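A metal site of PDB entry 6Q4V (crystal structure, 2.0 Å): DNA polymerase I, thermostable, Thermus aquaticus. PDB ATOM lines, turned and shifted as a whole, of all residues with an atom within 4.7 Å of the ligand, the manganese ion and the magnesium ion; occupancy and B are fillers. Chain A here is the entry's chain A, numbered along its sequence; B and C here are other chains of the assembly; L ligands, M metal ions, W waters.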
ATOM      1  N   ARG A 282      17.347  -3.054 -14.964  1.00  0.00           N
ATOM      2  CA  ARG A 282      18.741  -2.874 -14.598  1.00  0.00           C
ATOM      3  C   ARG A 282      18.998  -1.428 -14.207  1.00  0.00           C
ATOM      4  O   ARG A 282      18.272  -0.500 -14.584  1.00  0.00           O
ATOM      5  CB  ARG A 282      19.654  -3.245 -15.763  1.00  0.00           C
ATOM      6  CG  ARG A 282      19.938  -4.725 -15.941  1.00  0.00           C
ATOM      7  CD  ARG A 282      21.082  -4.899 -16.931  1.00  0.00           C
ATOM      8  NE  ARG A 282      21.578  -6.273 -17.005  1.00  0.00           N
ATOM      9  CZ  ARG A 282      22.549  -6.658 -17.829  1.00  0.00           C
ATOM     10  NH1 ARG A 282      23.111  -5.792 -18.657  1.00  0.00           N
ATOM     11  NH2 ARG A 282      22.942  -7.923 -17.828  1.00  0.00           N
ATOM     12  N   ASP A 319      29.904 -12.024  -7.195  1.00  0.00           N
ATOM     13  CA  ASP A 319      29.342 -12.141  -8.537  1.00  0.00           C
ATOM     14  C   ASP A 319      28.525 -13.416  -8.619  1.00  0.00           C
ATOM     15  O   ASP A 319      29.066 -14.508  -8.404  1.00  0.00           O
ATOM     16  CB  ASP A 319      30.460 -12.133  -9.584  1.00  0.00           C
ATOM     17  CG  ASP A 319      29.933 -12.123 -11.011  1.00  0.00           C
ATOM     18  OD1 ASP A 319      29.105 -12.987 -11.361  1.00  0.00           O
ATOM     19  OD2 ASP A 319      30.355 -11.238 -11.785  1.00  0.00           O
ATOM     20  N   TYR A 320      27.238 -13.285  -8.955  1.00  0.00           N
ATOM     21  CA  TYR A 320      26.383 -14.460  -9.094  1.00  0.00           C
ATOM     22  C   TYR A 320      26.895 -15.371 -10.196  1.00  0.00           C
ATOM     23  O   TYR A 320      27.392 -14.899 -11.227  1.00  0.00           O
ATOM     24  CB  TYR A 320      24.945 -14.041  -9.401  1.00  0.00           C
ATOM     25  CG  TYR A 320      24.156 -13.527  -8.217  1.00  0.00           C
ATOM     26  CD1 TYR A 320      23.666 -14.397  -7.249  1.00  0.00           C
ATOM     27  CD2 TYR A 320      23.873 -12.173  -8.077  1.00  0.00           C
ATOM     28  CE1 TYR A 320      22.935 -13.939  -6.165  1.00  0.00           C
ATOM     29  CE2 TYR A 320      23.146 -11.704  -7.001  1.00  0.00           C
ATOM     30  CZ  TYR A 320      22.679 -12.592  -6.055  1.00  0.00           C
ATOM     31  OH  TYR A 320      21.952 -12.123  -4.979  1.00  0.00           O
ATOM     32  N   SER A 321      26.766 -16.674  -9.994  1.00  0.00           N
ATOM     33  CA  SER A 321      27.199 -17.665 -10.975  1.00  0.00           C
ATOM     34  C   SER A 321      26.081 -17.920 -11.989  1.00  0.00           C
ATOM     35  O   SER A 321      24.940 -18.204 -11.605  1.00  0.00           O
ATOM     36  CB  SER A 321      27.598 -18.967 -10.283  1.00  0.00           C
ATOM     37  OG  SER A 321      26.995 -20.085 -10.920  1.00  0.00           O
ATOM     38  N   GLN A 322      26.422 -17.820 -13.270  1.00  0.00           N
ATOM     39  CA  GLN A 322      25.527 -18.179 -14.370  1.00  0.00           C
ATOM     40  C   GLN A 322      24.111 -17.654 -14.128  1.00  0.00           C
ATOM     41  O   GLN A 322      23.125 -18.386 -14.238  1.00  0.00           O
ATOM     42  CB  GLN A 322      25.494 -19.687 -14.579  1.00  0.00           C
ATOM     43  CG  GLN A 322      26.845 -20.380 -14.579  1.00  0.00           C
ATOM     44  CD  GLN A 322      26.704 -21.893 -14.566  1.00  0.00           C
ATOM     45  OE1 GLN A 322      27.209 -22.568 -13.670  1.00  0.00           O
ATOM     46  NE2 GLN A 322      26.005 -22.422 -15.569  1.00  0.00           N
ATOM     47  N   ILE A 323      24.007 -16.366 -13.806  1.00  0.00           N
ATOM     48  CA  ILE A 323      22.818 -15.885 -13.108  1.00  0.00           C
ATOM     49  C   ILE A 323      21.567 -16.040 -13.967  1.00  0.00           C
ATOM     50  O   ILE A 323      20.579 -16.643 -13.545  1.00  0.00           O
ATOM     51  CB  ILE A 323      23.017 -14.439 -12.616  1.00  0.00           C
ATOM     52  CG1 ILE A 323      21.795 -14.004 -11.793  1.00  0.00           C
ATOM     53  CG2 ILE A 323      23.250 -13.481 -13.773  1.00  0.00           C
ATOM     54  CD1 ILE A 323      21.458 -14.949 -10.655  1.00  0.00           C
ATOM     55  N   GLU A 324      21.584 -15.495 -15.196  1.00  0.00           N
ATOM     56  CA  GLU A 324      20.358 -15.517 -15.987  1.00  0.00           C
ATOM     57  C   GLU A 324      19.995 -16.920 -16.452  1.00  0.00           C
ATOM     58  O   GLU A 324      18.839 -17.158 -16.797  1.00  0.00           O
ATOM     59  CB  GLU A 324      20.483 -14.554 -17.172  1.00  0.00           C
ATOM     60  CG  GLU A 324      20.135 -13.108 -16.777  1.00  0.00           C
ATOM     61  CD  GLU A 324      20.279 -12.106 -17.906  1.00  0.00           C
ATOM     62  OE1 GLU A 324      19.933 -12.435 -19.067  1.00  0.00           O
ATOM     63  OE2 GLU A 324      20.734 -10.978 -17.640  1.00  0.00           O
ATOM     64  N   HIS A 348      28.794 -22.570 -19.019  1.00  0.00           N
ATOM     65  CA  HIS A 348      29.799 -21.755 -19.695  1.00  0.00           C
ATOM     66  C   HIS A 348      31.094 -22.533 -19.868  1.00  0.00           C
ATOM     67  O   HIS A 348      31.720 -22.481 -20.935  1.00  0.00           O
ATOM     68  CB  HIS A 348      30.039 -20.462 -18.911  1.00  0.00           C
ATOM     69  CG  HIS A 348      28.812 -19.622 -18.761  1.00  0.00           C
ATOM     70  ND1 HIS A 348      27.795 -19.613 -19.700  1.00  0.00           N
ATOM     71  CD2 HIS A 348      28.424 -18.758 -17.786  1.00  0.00           C
ATOM     72  CE1 HIS A 348      26.850 -18.779 -19.311  1.00  0.00           C
ATOM     73  NE2 HIS A 348      27.199 -18.256 -18.155  1.00  0.00           N
ATOM     74  N   ARG A 368      36.240 -19.212 -21.365  1.00  0.00           N
ATOM     75  CA  ARG A 368      34.901 -19.189 -20.777  1.00  0.00           C
ATOM     76  C   ARG A 368      34.174 -17.893 -21.125  1.00  0.00           C
ATOM     77  O   ARG A 368      32.951 -17.893 -21.327  1.00  0.00           O
ATOM     78  CB  ARG A 368      35.009 -19.364 -19.257  1.00  0.00           C
ATOM     79  CG  ARG A 368      33.722 -19.809 -18.590  1.00  0.00           C
ATOM     80  CD  ARG A 368      33.977 -20.222 -17.144  1.00  0.00           C
ATOM     81  NE  ARG A 368      32.748 -20.302 -16.368  1.00  0.00           N
ATOM     82  CZ  ARG A 368      32.105 -19.251 -15.852  1.00  0.00           C
ATOM     83  NH1 ARG A 368      32.582 -18.030 -16.027  1.00  0.00           N
ATOM     84  NH2 ARG A 368      30.992 -19.433 -15.161  1.00  0.00           N
ATOM     85  N   LYS A 372      30.300 -17.593 -22.973  1.00  0.00           N
ATOM     86  CA  LYS A 372      29.130 -16.876 -22.476  1.00  0.00           C
ATOM     87  C   LYS A 372      28.388 -16.192 -23.611  1.00  0.00           C
ATOM     88  O   LYS A 372      27.162 -16.291 -23.715  1.00  0.00           O
ATOM     89  CB  LYS A 372      29.534 -15.862 -21.407  1.00  0.00           C
ATOM     90  CG  LYS A 372      29.659 -16.453 -20.023  1.00  0.00           C
ATOM     91  CD  LYS A 372      29.645 -15.374 -18.953  1.00  0.00           C
ATOM     92  CE  LYS A 372      31.004 -15.215 -18.306  1.00  0.00           C
ATOM     93  NZ  LYS A 372      30.936 -14.314 -17.128  1.00  0.00           N
ATOM     94  N   THR A 373      29.117 -15.470 -24.459  1.00  0.00           N
ATOM     95  CA  THR A 373      28.481 -14.839 -25.611  1.00  0.00           C
ATOM     96  C   THR A 373      27.701 -15.860 -26.426  1.00  0.00           C
ATOM     97  O   THR A 373      26.580 -15.598 -26.878  1.00  0.00           O
ATOM     98  CB  THR A 373      29.532 -14.150 -26.477  1.00  0.00           C
ATOM     99  OG1 THR A 373      30.386 -13.346 -25.651  1.00  0.00           O
ATOM    100  CG2 THR A 373      28.877 -13.263 -27.525  1.00  0.00           C
ATOM    101  N   PHE A 376      24.499 -17.134 -24.321  1.00  0.00           N
ATOM    102  CA  PHE A 376      23.456 -16.122 -24.240  1.00  0.00           C
ATOM    103  C   PHE A 376      23.029 -15.635 -25.625  1.00  0.00           C
ATOM    104  O   PHE A 376      21.872 -15.261 -25.809  1.00  0.00           O
ATOM    105  CB  PHE A 376      23.920 -14.956 -23.363  1.00  0.00           C
ATOM    106  CG  PHE A 376      24.115 -15.332 -21.922  1.00  0.00           C
ATOM    107  CD1 PHE A 376      23.042 -15.770 -21.154  1.00  0.00           C
ATOM    108  CD2 PHE A 376      25.365 -15.274 -21.328  1.00  0.00           C
ATOM    109  CE1 PHE A 376      23.214 -16.132 -19.832  1.00  0.00           C
ATOM    110  CE2 PHE A 376      25.546 -15.639 -20.006  1.00  0.00           C
ATOM    111  CZ  PHE A 376      24.468 -16.063 -19.247  1.00  0.00           C
ATOM    112  N   TYR A 380      19.015 -16.025 -26.575  1.00  0.00           N
ATOM    113  CA  TYR A 380      18.200 -14.870 -26.900  1.00  0.00           C
ATOM    114  C   TYR A 380      17.994 -14.700 -28.399  1.00  0.00           C
ATOM    115  O   TYR A 380      17.535 -13.635 -28.840  1.00  0.00           O
ATOM    116  CB  TYR A 380      18.815 -13.615 -26.275  1.00  0.00           C
ATOM    117  CG  TYR A 380      18.763 -13.679 -24.760  1.00  0.00           C
ATOM    118  CD1 TYR A 380      17.565 -13.877 -24.101  1.00  0.00           C
ATOM    119  CD2 TYR A 380      19.924 -13.574 -23.988  1.00  0.00           C
ATOM    120  CE1 TYR A 380      17.501 -13.950 -22.729  1.00  0.00           C
ATOM    121  CE2 TYR A 380      19.872 -13.644 -22.605  1.00  0.00           C
ATOM    122  CZ  TYR A 380      18.656 -13.829 -21.985  1.00  0.00           C
ATOM    123  OH  TYR A 380      18.569 -13.905 -20.602  1.00  0.00           O
ATOM    124  N   VAL A 492      27.645  -3.951 -10.591  1.00  0.00           N
ATOM    125  CA  VAL A 492      27.808  -4.183 -12.025  1.00  0.00           C
ATOM    126  C   VAL A 492      26.816  -5.253 -12.451  1.00  0.00           C
ATOM    127  O   VAL A 492      27.197  -6.353 -12.851  1.00  0.00           O
ATOM    128  CB  VAL A 492      29.260  -4.578 -12.370  1.00  0.00           C
ATOM    129  CG1 VAL A 492      29.459  -4.631 -13.871  1.00  0.00           C
ATOM    130  CG2 VAL A 492      30.240  -3.594 -11.743  1.00  0.00           C
ATOM    131  N   ASP A 494      25.153  -7.921 -11.943  1.00  0.00           N
ATOM    132  CA  ASP A 494      25.058  -9.103 -11.100  1.00  0.00           C
ATOM    133  C   ASP A 494      26.239  -9.215 -10.145  1.00  0.00           C
ATOM    134  O   ASP A 494      26.514 -10.291  -9.624  1.00  0.00           O
ATOM    135  CB  ASP A 494      24.924 -10.366 -11.952  1.00  0.00           C
ATOM    136  CG  ASP A 494      26.253 -10.875 -12.463  1.00  0.00           C
ATOM    137  OD1 ASP A 494      27.149 -10.046 -12.723  1.00  0.00           O
ATOM    138  OD2 ASP A 494      26.415 -12.105 -12.576  1.00  0.00           O
ATOM    139  N   GLU A 495      26.943  -8.109  -9.914  1.00  0.00           N
ATOM    140  CA  GLU A 495      28.155  -8.096  -9.104  1.00  0.00           C
ATOM    141  C   GLU A 495      28.106  -6.901  -8.149  1.00  0.00           C
ATOM    142  O   GLU A 495      27.573  -5.851  -8.481  1.00  0.00           O
ATOM    143  CB  GLU A 495      29.403  -8.030 -10.002  1.00  0.00           C
ATOM    144  CG  GLU A 495      30.714  -7.765  -9.261  1.00  0.00           C
ATOM    145  CD  GLU A 495      31.880  -7.548 -10.220  1.00  0.00           C
ATOM    146  OE1 GLU A 495      31.642  -7.574 -11.452  1.00  0.00           O
ATOM    147  OE2 GLU A 495      33.013  -7.360  -9.749  1.00  0.00           O
ATOM    148  N   LYS A 540      38.724 -11.016  -7.844  1.00  0.00           N
ATOM    149  CA  LYS A 540      37.912 -11.964  -8.609  1.00  0.00           C
ATOM    150  C   LYS A 540      38.764 -13.117  -9.100  1.00  0.00           C
ATOM    151  O   LYS A 540      39.162 -13.983  -8.320  1.00  0.00           O
ATOM    152  CB  LYS A 540      37.226 -11.265  -9.792  1.00  0.00           C
ATOM    153  CG  LYS A 540      36.086 -10.331  -9.388  1.00  0.00           C
ATOM    154  CD  LYS A 540      35.321  -9.772 -10.579  1.00  0.00           C
ATOM    155  CE  LYS A 540      34.366 -10.802 -11.182  1.00  0.00           C
ATOM    156  NZ  LYS A 540      33.291 -10.183 -12.011  1.00  0.00           N
ATOM    157  P    DT B   4      21.620 -12.279 -34.936  1.00  0.00           P
ATOM    158  OP1  DT B   4      22.691 -11.283 -35.206  1.00  0.00           O
ATOM    159  OP2  DT B   4      21.706 -13.622 -35.537  1.00  0.00           O
ATOM    160  O5'  DT B   4      21.470 -12.485 -33.358  1.00  0.00           O
ATOM    161  C5'  DT B   4      21.217 -11.377 -32.514  1.00  0.00           C
ATOM    162  C4'  DT B   4      20.514 -11.805 -31.244  1.00  0.00           C
ATOM    163  O4'  DT B   4      21.370 -12.734 -30.515  1.00  0.00           O
ATOM    164  C3'  DT B   4      20.229 -10.687 -30.277  1.00  0.00           C
ATOM    165  O3'  DT B   4      19.001 -10.016 -30.593  1.00  0.00           O
ATOM    166  C2'  DT B   4      20.189 -11.409 -28.950  1.00  0.00           C
ATOM    167  C1'  DT B   4      21.251 -12.493 -29.121  1.00  0.00           C
ATOM    168  N1   DT B   4      22.598 -12.111 -28.566  1.00  0.00           N
ATOM    169  C2   DT B   4      22.762 -11.940 -27.203  1.00  0.00           C
ATOM    170  O2   DT B   4      21.865 -12.085 -26.399  1.00  0.00           O
ATOM    171  N3   DT B   4      24.041 -11.595 -26.814  1.00  0.00           N
ATOM    172  C4   DT B   4      25.133 -11.421 -27.627  1.00  0.00           C
ATOM    173  O4   DT B   4      26.239 -11.108 -27.190  1.00  0.00           O
ATOM    174  C5   DT B   4      24.890 -11.617 -29.043  1.00  0.00           C
ATOM    175  C7   DT B   4      26.005 -11.441 -30.026  1.00  0.00           C
ATOM    176  C6   DT B   4      23.660 -11.950 -29.430  1.00  0.00           C
ATOM    177  P    DG B   5      18.929  -8.413 -30.613  1.00  0.00           P
ATOM    178  OP1  DG B   5      17.666  -8.040 -31.290  1.00  0.00           O
ATOM    179  OP2  DG B   5      20.233  -7.899 -31.109  1.00  0.00           O
ATOM    180  O5'  DG B   5      18.776  -8.014 -29.066  1.00  0.00           O
ATOM    181  C5'  DG B   5      17.580  -8.371 -28.368  1.00  0.00           C
ATOM    182  C4'  DG B   5      17.820  -8.435 -26.865  1.00  0.00           C
ATOM    183  O4'  DG B   5      18.920  -9.334 -26.568  1.00  0.00           O
ATOM    184  C3'  DG B   5      18.216  -7.134 -26.222  1.00  0.00           C
ATOM    185  O3'  DG B   5      17.084  -6.312 -25.984  1.00  0.00           O
ATOM    186  C2'  DG B   5      18.880  -7.607 -24.948  1.00  0.00           C
ATOM    187  C1'  DG B   5      19.576  -8.886 -25.394  1.00  0.00           C
ATOM    188  N9   DG B   5      20.996  -8.676 -25.680  1.00  0.00           N
ATOM    189  C8   DG B   5      21.613  -8.675 -26.915  1.00  0.00           C
ATOM    190  N7   DG B   5      22.897  -8.454 -26.845  1.00  0.00           N
ATOM    191  C5   DG B   5      23.142  -8.295 -25.484  1.00  0.00           C
ATOM    192  C6   DG B   5      24.345  -8.023 -24.792  1.00  0.00           C
ATOM    193  O6   DG B   5      25.488  -7.881 -25.266  1.00  0.00           O
ATOM    194  N1   DG B   5      24.139  -7.940 -23.417  1.00  0.00           N
ATOM    195  C2   DG B   5      22.938  -8.088 -22.792  1.00  0.00           C
ATOM    196  N2   DG B   5      22.939  -7.967 -21.455  1.00  0.00           N
ATOM    197  N3   DG B   5      21.801  -8.340 -23.432  1.00  0.00           N
ATOM    198  C4   DG B   5      21.976  -8.426 -24.766  1.00  0.00           C
ATOM    199  N1  DOC C  12      27.346  -7.519 -19.432  1.00  0.00           N
ATOM    200  C2  DOC C  12      26.278  -7.605 -20.393  1.00  0.00           C
ATOM    201  N3  DOC C  12      26.603  -7.896 -21.806  1.00  0.00           N
ATOM    202  C4  DOC C  12      27.842  -8.089 -22.194  1.00  0.00           C
ATOM    203  C5  DOC C  12      28.964  -8.010 -21.173  1.00  0.00           C
ATOM    204  C6  DOC C  12      28.663  -7.731 -19.833  1.00  0.00           C
ATOM    205  O2  DOC C  12      24.989  -7.404 -19.994  1.00  0.00           O
ATOM    206  N4  DOC C  12      28.134  -8.359 -23.573  1.00  0.00           N
ATOM    207  C1' DOC C  12      27.083  -7.207 -18.037  1.00  0.00           C
ATOM    208  C2' DOC C  12      26.686  -8.430 -17.257  1.00  0.00           C
ATOM    209  C3' DOC C  12      27.932  -8.757 -16.452  1.00  0.00           C
ATOM    210  C4' DOC C  12      28.591  -7.399 -16.338  1.00  0.00           C
ATOM    211  O4' DOC C  12      28.198  -6.654 -17.468  1.00  0.00           O
ATOM    212  C5' DOC C  12      30.042  -7.377 -16.276  1.00  0.00           C
ATOM    213  O5' DOC C  12      30.624  -8.065 -17.390  1.00  0.00           O
ATOM    214  P   DOC C  12      32.177  -7.971 -17.540  1.00  0.00           P
ATOM    215  OP1 DOC C  12      32.827  -8.312 -16.148  1.00  0.00           O
ATOM    216  OP2 DOC C  12      32.655  -8.953 -18.571  1.00  0.00           O
HETATM  217  P1  LIG L   1      29.543 -16.136 -14.322  1.00  0.00           P
HETATM  218  O1  LIG L   1      29.295 -15.036 -13.337  1.00  0.00           O
HETATM  219  O2  LIG L   1      29.375 -17.537 -13.739  1.00  0.00           O
HETATM  220  O3  LIG L   1      30.937 -16.043 -14.965  1.00  0.00           O
HETATM  221  P2  LIG L   1      27.199 -15.128 -15.684  1.00  0.00           P
HETATM  222  O4  LIG L   1      26.639 -14.681 -14.380  1.00  0.00           O
HETATM  223  O5  LIG L   1      26.215 -15.869 -16.571  1.00  0.00           O
HETATM  224  O6  LIG L   1      28.494 -16.037 -15.511  1.00  0.00           O
HETATM  225  P3  LIG L   1      28.136 -12.420 -16.110  1.00  0.00           P
HETATM  226  O7  LIG L   1      28.280 -12.286 -14.651  1.00  0.00           O
HETATM  227  O8  LIG L   1      29.353 -11.992 -16.920  1.00  0.00           O
HETATM  228  O9  LIG L   1      27.784 -13.910 -16.526  1.00  0.00           O
HETATM  229  O10 LIG L   1      26.889 -11.600 -16.669  1.00  0.00           O
HETATM  230  C1  LIG L   1      25.655 -11.477 -15.927  1.00  0.00           C
HETATM  231  C2  LIG L   1      24.493 -11.749 -16.842  1.00  0.00           C
HETATM  232  O11 LIG L   1      24.479 -10.796 -17.926  1.00  0.00           O
HETATM  233  C3  LIG L   1      24.490 -13.110 -17.526  1.00  0.00           C
HETATM  234  O12 LIG L   1      23.907 -14.110 -16.685  1.00  0.00           O
HETATM  235  C4  LIG L   1      23.604 -12.847 -18.735  1.00  0.00           C
HETATM  236  C5  LIG L   1      23.912 -11.404 -19.082  1.00  0.00           C
HETATM  237  N1  LIG L   1      24.854 -11.260 -20.189  1.00  0.00           N
HETATM  238  C6  LIG L   1      26.224 -11.226 -20.134  1.00  0.00           C
HETATM  239  N2  LIG L   1      26.806 -11.241 -21.301  1.00  0.00           N
HETATM  240  C7  LIG L   1      25.748 -11.286 -22.197  1.00  0.00           C
HETATM  241  C8  LIG L   1      25.689 -11.353 -23.597  1.00  0.00           C
HETATM  242  N3  LIG L   1      26.764 -11.437 -24.383  1.00  0.00           N
HETATM  243  N4  LIG L   1      24.464 -11.380 -24.176  1.00  0.00           N
HETATM  244  C9  LIG L   1      23.388 -11.349 -23.398  1.00  0.00           C
HETATM  245  N5  LIG L   1      23.315 -11.306 -22.060  1.00  0.00           N
HETATM  246  C10 LIG L   1      24.536 -11.283 -21.521  1.00  0.00           C
HETATM  247 MN    MN M   1      27.739 -13.580 -12.932  1.00  0.00          MN
HETATM  248 MG    MG M   2      29.122 -10.336 -13.371  1.00  0.00          MG
HETATM  249  O   HOH W   1      31.639 -13.221 -14.164  1.00  0.00           O
HETATM  250  O   HOH W   2      31.022 -10.633 -15.160  1.00  0.00           O
HETATM  251  O   HOH W   3      29.543 -11.749 -21.620  1.00  0.00           O
HETATM  252  O   HOH W   4      29.538  -7.997 -13.146  1.00  0.00           O
HETATM  253  O   HOH W   5      31.019 -11.084 -19.264  1.00  0.00           O
HETATM  254  O   HOH W   6      30.315 -15.442 -10.937  1.00  0.00           O
HETATM  255  O   HOH W   7      20.438 -10.389 -20.909  1.00  0.00           O
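The manganese ion is bound by OD2 of Asp 494 (2.0 Å), O4 of the ligand (2.1 Å), OD1 of Asp 319 (2.2 Å), O1 of the ligand (2.2 Å), O of Tyr 320 (2.2 Å) and O7 of the ligand (2.2 Å). The manganese ion has six donor atoms within binding distance.
The side-chain carboxylate (OD2) of Asp 319 lies close to the side-chain amino group (NZ) of Lys 540 (3.1 Å). O2 of DOC 12 of chain C lies within hydrogen-bond range of the guanidinium group (NH1) of Arg 282 (2.8 Å). O2 of DOC 12 of chain C sits close to N2 of DG 5 of chain B, at 2.6 Å. NH2 of Arg 282 is in salt-bridge range of OE2 of Glu 324. OH of Tyr 380 lies within hydrogen-bond range of OE1 of Glu 324 (2.5 Å).
Merely in contact with the magnesium ion: DOC 12 of chain C (3.7 Å). Three residues have an atom within 4 Å of the magnesium ion: Asp 319, Asp 494 and DOC 12 of chain C. The nearest printed residue that does not touch the magnesium ion is Glu 495 (4.1 Å).
The magnesium ion is bound by OD1 of Asp 494, at 2.1 Å. The magnesium ion is bound by the side-chain carboxylate (OD2) of Asp 319 (2.2 Å). Water W4 is bound to the magnesium ion (2.4 Å). An oxygen (O7) of the ligand is bound to the magnesium ion. The magnesium ion has four donor atoms within binding distance. Slightly farther from the magnesium ion lies water W2 (2.6 Å).
N2 of DG 5 of chain B sits close to N5 of the ligand (3.4 Å). CA of Ser 321 touches O2 of the ligand, 3.5 Å away. Phe 376 touches the ligand. Hydrophobic or aromatic side chains that line the ligand: Ile 323, His 348 and Phe 376. 15 residues have an atom within 4 Å of the ligand: Arg 282, Asp 319, Tyr 320, Ser 321, Gln 322, Ile 323, Glu 324, His 348, Arg 368, Lys 372, Phe 376, Asp 494, DT 4 of chain B, DG 5 of chain B and DOC 12 of chain C. Along chain A the residues within 4 Å of the ligand span positions 282 to 494.
Within 4 Å of the manganese ion: Asp 319, Tyr 320 and Asp 494.
Water W4 lies within hydrogen-bond range of OE1 of Glu 495 and O of Val 492. Water W2 lies within hydrogen-bond range of an oxygen (O8) of the ligand (2.8 Å) and OP1 of DOC 12 of chain C (3.1 Å). Water W5 bridges OP2 of DOC 12 of chain C (2.8 Å) and O8 of the ligand (3.0 Å). Water W1 lies within hydrogen-bond range of O3 of the ligand (3.0 Å) and NZ of Lys 372 (3.2 Å). Water W7 bridges the side-chain carboxylate (OE1) of Glu 324 (2.8 Å) and a nitrogen (N5) of the ligand (3.2 Å).
O4 of DT 4 of chain B is in hydrogen-bond range of a nitrogen (N3) of the ligand (2.9 Å). The side-chain amino group of Lys 372 lies within salt-bridge range of an oxygen (O3) of the ligand, 2.8 Å away. An oxygen (O3) of the ligand is in salt-bridge range of the guanidinium group (NH1) of Arg 368, at 2.8 Å. O2 of the ligand is in hydrogen-bond range of N of Gln 322, at 3.0 Å. A ring nitrogen (NE2) of His 348 lies within hydrogen-bond range of an oxygen (O5) of the ligand (3.0 Å). A nitrogen (N3) of the ligand is in hydrogen-bond range of N4 of DOC 12 of chain C. The backbone NH of Ile 323 lies close to an oxygen (O4) of the ligand, 3.2 Å away. The backbone NH (N) of Glu 324 sits at hydrogen-bond distance from an oxygen (O12) of the ligand (3.1 Å). The guanidinium group (NH2) of Arg 282 lies within hydrogen-bond range of an oxygen (O11) of the ligand (3.3 Å).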
